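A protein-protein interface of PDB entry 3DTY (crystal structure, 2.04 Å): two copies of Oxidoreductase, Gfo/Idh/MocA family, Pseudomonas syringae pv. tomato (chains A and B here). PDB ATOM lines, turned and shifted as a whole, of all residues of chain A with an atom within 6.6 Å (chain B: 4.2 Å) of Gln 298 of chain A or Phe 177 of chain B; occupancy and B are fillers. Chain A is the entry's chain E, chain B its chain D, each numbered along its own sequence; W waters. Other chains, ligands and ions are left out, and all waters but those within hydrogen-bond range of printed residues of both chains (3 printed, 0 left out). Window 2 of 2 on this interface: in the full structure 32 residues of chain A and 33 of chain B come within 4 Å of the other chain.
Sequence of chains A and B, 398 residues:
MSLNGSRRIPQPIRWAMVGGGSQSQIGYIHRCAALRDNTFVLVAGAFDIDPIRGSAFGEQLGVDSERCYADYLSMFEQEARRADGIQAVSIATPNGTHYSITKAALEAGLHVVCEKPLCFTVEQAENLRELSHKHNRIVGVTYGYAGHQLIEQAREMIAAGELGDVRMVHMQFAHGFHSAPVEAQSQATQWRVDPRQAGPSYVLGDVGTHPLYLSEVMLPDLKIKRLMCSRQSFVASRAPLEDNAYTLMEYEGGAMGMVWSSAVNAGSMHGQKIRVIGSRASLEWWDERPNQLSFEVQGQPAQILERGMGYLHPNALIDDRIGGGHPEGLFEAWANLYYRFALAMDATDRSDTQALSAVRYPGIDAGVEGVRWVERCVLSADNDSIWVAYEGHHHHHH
Water W3 bridges O of Gly 267 of chain B (2.8 Å) and O of Gln 300 of chain A (3.4 Å).
Water W2 lies within hydrogen-bond range of the side-chain amide nitrogen (NE2) of Gln 298 of chain A, the backbone carbonyl oxygen (O) of Ser 268 of chain B and the side-chain sulfur (SD) of Met 269 of chain B.
Water W1 lies within hydrogen-bond range of the backbone carbonyl oxygen of Gln 300 of chain A (3.2 Å) and the side-chain sulfur of Met 269 of chain B (3.6 Å).
Printed residues of chain B within 4 Å of Ser 279 of chain A: Ser 179.
Of the printed residues of chain B, Ser 282 of chain A touches Ala 266.
Printed residues of chain B within 4 Å of Glu 296 of chain A: Ala 266 (3.7 Å) and Gly 267 (3.4 Å).
Of chain B, only Gly 176, Phe 177, Ala 266 and Gly 267 come within 4 Å of Gln 298 of chain A.
His 175 of chain B touches none of the printed residues of chain A.
His 178 of chain B touches none of the printed residues of chain A.
Of the printed residues of chain A, Ser 179 of chain B touches Ser 279 (3.6 Å).
The nearest residue of chain B that does not touch Gln 298 of chain A is Ser 268 of chain B (4.02 Å).
The nearest residue of chain A that does not touch Phe 177 of chain B is Gly 299 of chain A (6.4 Å).
No position is printed for both chains.
Ser 279 of chain A touches Ser 179 of chain B.
CB of Ala 266 of chain B touches CA of Ala 281 of chain A, 3.8 Å away.
Glu 296 of chain A touches Ala 266 of chain B.
Glu 296 of chain A touches Gly 267 of chain B (CB to CA, 3.4 Å).
Gln 298 of chain A touches Phe 177 of chain B (NE2 to CA, 3.6 Å).
Ala 266 of chain B touches Gln 298 of chain A.
Of the 10 printed residues of chain B, 5 touch a printed residue of chain A.
Hydrophobic or aromatic side chains of chain B within 4 Å of the printed part of chain A: Phe 177 and Ala 266.
Among the printed residues, no Asp or Glu carboxylate lies within 4 Å of a Lys or Arg side-chain nitrogen of the other chain.
The backbone carbonyl oxygen (O) of Gly 176 of chain B lies close to the side-chain amide oxygen (OE1) of Gln 298 of chain A.
The backbone carbonyl oxygen of Ala 266 of chain B lies within hydrogen-bond range of the side-chain hydroxyl of Ser 282 of chain A.
N of Gly 267 of chain B lies within hydrogen-bond range of OE1 of Gln 298 of chain A (2.8 Å).
N of Phe 177 of chain B lies within hydrogen-bond range of ND1 of His 175 of chain B, 3.1 Å away.
The backbone carbonyl oxygen (O) of Gly 176 of chain B lies within hydrogen-bond range of the side-chain hydroxyl (OG) of Ser 179 of chain B (2.7 Å).
The backbone carbonyl oxygen (O) of Ser 268 of chain B lies within hydrogen-bond range of the backbone NH (N) of Gly 176 of chain B (3.0 Å).
The backbone carbonyl oxygen (O) of Ala 263 of chain B lies within hydrogen-bond range of the backbone NH (N) of Ser 179 of chain B, 3.5 Å away.
O of Arg 280 of chain A sits at hydrogen-bond distance from N of Gln 298 of chain A, at 3.1 Å.
O of Ser 282 of chain A lies within hydrogen-bond range of N of Glu 296 of chain A (2.8 Å).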
ATOM      1  N   SER A 279       0.539  11.110  -1.327  1.00  0.00           N
ATOM      2  CA  SER A 279       0.141  10.203  -0.261  1.00  0.00           C
ATOM      3  C   SER A 279       1.122   9.041  -0.103  1.00  0.00           C
ATOM      4  O   SER A 279       1.228   8.465   0.972  1.00  0.00           O
ATOM      5  CB  SER A 279      -1.258   9.653  -0.541  1.00  0.00           C
ATOM      6  OG  SER A 279      -1.285   8.960  -1.779  1.00  0.00           O
ATOM      7  N   ARG A 280       1.833   8.708  -1.177  1.00  0.00           N
ATOM      8  CA  ARG A 280       2.778   7.596  -1.166  1.00  0.00           C
ATOM      9  C   ARG A 280       4.246   7.998  -1.065  1.00  0.00           C
ATOM     10  O   ARG A 280       5.041   7.321  -0.411  1.00  0.00           O
ATOM     11  CB  ARG A 280       2.585   6.741  -2.429  1.00  0.00           C
ATOM     12  CG  ARG A 280       3.681   5.706  -2.662  1.00  0.00           C
ATOM     13  CD  ARG A 280       3.318   4.710  -3.761  1.00  0.00           C
ATOM     14  NE  ARG A 280       4.310   3.642  -3.883  1.00  0.00           N
ATOM     15  CZ  ARG A 280       5.442   3.744  -4.574  1.00  0.00           C
ATOM     16  NH1 ARG A 280       5.731   4.866  -5.220  1.00  0.00           N
ATOM     17  NH2 ARG A 280       6.289   2.724  -4.614  1.00  0.00           N
ATOM     18  N   ALA A 281       4.605   9.097  -1.717  1.00  0.00           N
ATOM     19  CA  ALA A 281       5.987   9.537  -1.726  1.00  0.00           C
ATOM     20  C   ALA A 281       6.107  11.000  -2.111  1.00  0.00           C
ATOM     21  O   ALA A 281       5.130  11.637  -2.502  1.00  0.00           O
ATOM     22  CB  ALA A 281       6.775   8.694  -2.708  1.00  0.00           C
ATOM     23  N   SER A 282       7.324  11.517  -2.006  1.00  0.00           N
ATOM     24  CA  SER A 282       7.600  12.896  -2.366  1.00  0.00           C
ATOM     25  C   SER A 282       8.787  12.926  -3.312  1.00  0.00           C
ATOM     26  O   SER A 282       9.543  11.950  -3.406  1.00  0.00           O
ATOM     27  CB  SER A 282       7.952  13.725  -1.127  1.00  0.00           C
ATOM     28  OG  SER A 282       6.864  13.833  -0.236  1.00  0.00           O
ATOM     29  N   GLU A 296      11.527  10.229  -2.455  1.00  0.00           N
ATOM     30  CA  GLU A 296      11.347   9.669  -1.126  1.00  0.00           C
ATOM     31  C   GLU A 296      10.004   8.973  -0.895  1.00  0.00           C
ATOM     32  O   GLU A 296       9.000   9.619  -0.587  1.00  0.00           O
ATOM     33  CB  GLU A 296      11.531  10.790  -0.098  1.00  0.00           C
ATOM     34  CG  GLU A 296      12.839  11.570  -0.254  1.00  0.00           C
ATOM     35  CD  GLU A 296      12.727  13.012   0.233  1.00  0.00           C
ATOM     36  OE1 GLU A 296      12.068  13.242   1.269  1.00  0.00           O
ATOM     37  OE2 GLU A 296      13.304  13.918  -0.414  1.00  0.00           O
ATOM     38  N   VAL A 297       9.999   7.653  -1.051  1.00  0.00           N
ATOM     39  CA  VAL A 297       8.800   6.860  -0.833  1.00  0.00           C
ATOM     40  C   VAL A 297       8.710   6.619   0.671  1.00  0.00           C
ATOM     41  O   VAL A 297       9.640   6.076   1.270  1.00  0.00           O
ATOM     42  CB  VAL A 297       8.882   5.493  -1.549  1.00  0.00           C
ATOM     43  CG1 VAL A 297       7.647   4.648  -1.204  1.00  0.00           C
ATOM     44  CG2 VAL A 297       8.999   5.697  -3.050  1.00  0.00           C
ATOM     45  N   GLN A 298       7.599   7.027   1.279  1.00  0.00           N
ATOM     46  CA  GLN A 298       7.421   6.855   2.711  1.00  0.00           C
ATOM     47  C   GLN A 298       7.609   5.399   3.117  1.00  0.00           C
ATOM     48  O   GLN A 298       7.002   4.502   2.531  1.00  0.00           O
ATOM     49  CB  GLN A 298       6.031   7.339   3.137  1.00  0.00           C
ATOM     50  CG  GLN A 298       5.758   7.237   4.636  1.00  0.00           C
ATOM     51  CD  GLN A 298       6.822   7.923   5.477  1.00  0.00           C
ATOM     52  OE1 GLN A 298       7.253   9.036   5.171  1.00  0.00           O
ATOM     53  NE2 GLN A 298       7.240   7.261   6.557  1.00  0.00           N
ATOM     54  N   GLY A 299       8.456   5.165   4.116  1.00  0.00           N
ATOM     55  CA  GLY A 299       8.691   3.804   4.568  1.00  0.00           C
ATOM     56  C   GLY A 299       9.745   3.043   3.775  1.00  0.00           C
ATOM     57  O   GLY A 299      10.007   1.876   4.043  1.00  0.00           O
ATOM     58  N   GLN A 300      10.340   3.696   2.788  1.00  0.00           N
ATOM     59  CA  GLN A 300      11.377   3.069   1.975  1.00  0.00           C
ATOM     60  C   GLN A 300      12.622   3.949   1.992  1.00  0.00           C
ATOM     61  O   GLN A 300      12.560   5.112   2.388  1.00  0.00           O
ATOM     62  CB  GLN A 300      10.910   2.908   0.528  1.00  0.00           C
ATOM     63  CG  GLN A 300       9.792   1.908   0.318  1.00  0.00           C
ATOM     64  CD  GLN A 300      10.188   0.514   0.736  1.00  0.00           C
ATOM     65  OE1 GLN A 300      11.181  -0.036   0.250  1.00  0.00           O
ATOM     66  NE2 GLN A 300       9.414  -0.073   1.645  1.00  0.00           N
ATOM     67  N   HIS B 175       7.281  15.373   9.132  1.00  0.00           N
ATOM     68  CA  HIS B 175       7.733  14.013   8.870  1.00  0.00           C
ATOM     69  C   HIS B 175       6.589  13.340   8.104  1.00  0.00           C
ATOM     70  O   HIS B 175       5.509  13.923   7.962  1.00  0.00           O
ATOM     71  CB  HIS B 175       7.998  13.290  10.195  1.00  0.00           C
ATOM     72  CG  HIS B 175       6.772  13.096  11.033  1.00  0.00           C
ATOM     73  ND1 HIS B 175       5.939  12.011  10.889  1.00  0.00           N
ATOM     74  CD2 HIS B 175       6.239  13.858  12.019  1.00  0.00           C
ATOM     75  CE1 HIS B 175       4.942  12.109  11.755  1.00  0.00           C
ATOM     76  NE2 HIS B 175       5.102  13.219  12.451  1.00  0.00           N
ATOM     77  N   GLY B 176       6.810  12.123   7.612  1.00  0.00           N
ATOM     78  CA  GLY B 176       5.758  11.454   6.861  1.00  0.00           C
ATOM     79  C   GLY B 176       5.236  10.136   7.411  1.00  0.00           C
ATOM     80  O   GLY B 176       4.517   9.420   6.715  1.00  0.00           O
ATOM     81  N   PHE B 177       5.560   9.822   8.661  1.00  0.00           N
ATOM     82  CA  PHE B 177       5.138   8.558   9.244  1.00  0.00           C
ATOM     83  C   PHE B 177       3.646   8.291   9.229  1.00  0.00           C
ATOM     84  O   PHE B 177       3.226   7.142   9.299  1.00  0.00           O
ATOM     85  CB  PHE B 177       5.684   8.423  10.671  1.00  0.00           C
ATOM     86  CG  PHE B 177       7.169   8.192  10.721  1.00  0.00           C
ATOM     87  CD1 PHE B 177       7.719   7.002  10.243  1.00  0.00           C
ATOM     88  CD2 PHE B 177       8.021   9.164  11.237  1.00  0.00           C
ATOM     89  CE1 PHE B 177       9.110   6.790  10.270  1.00  0.00           C
ATOM     90  CE2 PHE B 177       9.412   8.964  11.267  1.00  0.00           C
ATOM     91  CZ  PHE B 177       9.955   7.774  10.788  1.00  0.00           C
ATOM     92  N   HIS B 178       2.840   9.337   9.118  1.00  0.00           N
ATOM     93  CA  HIS B 178       1.400   9.136   9.095  1.00  0.00           C
ATOM     94  C   HIS B 178       0.761   9.487   7.763  1.00  0.00           C
ATOM     95  O   HIS B 178      -0.408   9.873   7.706  1.00  0.00           O
ATOM     96  CB  HIS B 178       0.762   9.921  10.233  1.00  0.00           C
ATOM     97  CG  HIS B 178       1.118   9.391  11.586  1.00  0.00           C
ATOM     98  ND1 HIS B 178       1.253  10.196  12.691  1.00  0.00           N
ATOM     99  CD2 HIS B 178       1.362   8.126  12.003  1.00  0.00           C
ATOM    100  CE1 HIS B 178       1.569   9.452  13.739  1.00  0.00           C
ATOM    101  NE2 HIS B 178       1.639   8.194  13.348  1.00  0.00           N
ATOM    102  N   SER B 179       1.534   9.343   6.691  1.00  0.00           N
ATOM    103  CA  SER B 179       1.032   9.637   5.356  1.00  0.00           C
ATOM    104  C   SER B 179      -0.088   8.654   5.034  1.00  0.00           C
ATOM    105  O   SER B 179      -0.979   8.951   4.237  1.00  0.00           O
ATOM    106  CB  SER B 179       2.154   9.512   4.318  1.00  0.00           C
ATOM    107  OG  SER B 179       3.210  10.421   4.594  1.00  0.00           O
ATOM    108  N   ALA B 263       2.633  15.536   9.441  1.00  0.00           N
ATOM    109  CA  ALA B 263       2.857  14.138   9.764  1.00  0.00           C
ATOM    110  C   ALA B 263       2.635  13.381   8.458  1.00  0.00           C
ATOM    111  O   ALA B 263       2.653  12.146   8.416  1.00  0.00           O
ATOM    112  CB  ALA B 263       1.870  13.684  10.828  1.00  0.00           C
ATOM    113  N   ALA B 266       5.514  12.806   3.253  1.00  0.00           N
ATOM    114  CA  ALA B 266       6.034  11.514   2.818  1.00  0.00           C
ATOM    115  C   ALA B 266       7.512  11.508   2.439  1.00  0.00           C
ATOM    116  O   ALA B 266       7.982  12.352   1.675  1.00  0.00           O
ATOM    117  CB  ALA B 266       5.194  10.977   1.661  1.00  0.00           C
ATOM    118  N   GLY B 267       8.230  10.533   2.987  1.00  0.00           N
ATOM    119  CA  GLY B 267       9.645  10.413   2.717  1.00  0.00           C
ATOM    120  C   GLY B 267      10.496  11.054   3.799  1.00  0.00           C
ATOM    121  O   GLY B 267      11.659  10.708   3.934  1.00  0.00           O
ATOM    122  N   SER B 268       9.922  11.981   4.566  1.00  0.00           N
ATOM    123  CA  SER B 268      10.651  12.666   5.633  1.00  0.00           C
ATOM    124  C   SER B 268      10.740  11.850   6.917  1.00  0.00           C
ATOM    125  O   SER B 268       9.727  11.379   7.439  1.00  0.00           O
ATOM    126  CB  SER B 268       9.999  14.022   5.937  1.00  0.00           C
ATOM    127  OG  SER B 268      10.682  14.703   6.979  1.00  0.00           O
ATOM    128  N   MET B 269      11.961  11.700   7.428  1.00  0.00           N
ATOM    129  CA  MET B 269      12.218  10.943   8.655  1.00  0.00           C
ATOM    130  C   MET B 269      11.926  11.744   9.924  1.00  0.00           C
ATOM    131  O   MET B 269      11.811  11.172  11.012  1.00  0.00           O
ATOM    132  CB  MET B 269      13.684  10.490   8.691  1.00  0.00           C
ATOM    133  CG  MET B 269      14.055   9.486   7.625  1.00  0.00           C
ATOM    134  SD  MET B 269      13.207   7.779   7.962  1.00  0.00           S
ATOM    135  CE  MET B 269      13.916   7.403   9.718  1.00  0.00           C
HETATM  136  O   HOH W   1      14.054   5.800   5.093  1.00  0.00           O
HETATM  137  O   HOH W   2       9.642   8.466   7.314  1.00  0.00           O
HETATM  138  O   HOH W   3      12.777   8.191   3.872  1.00  0.00           O
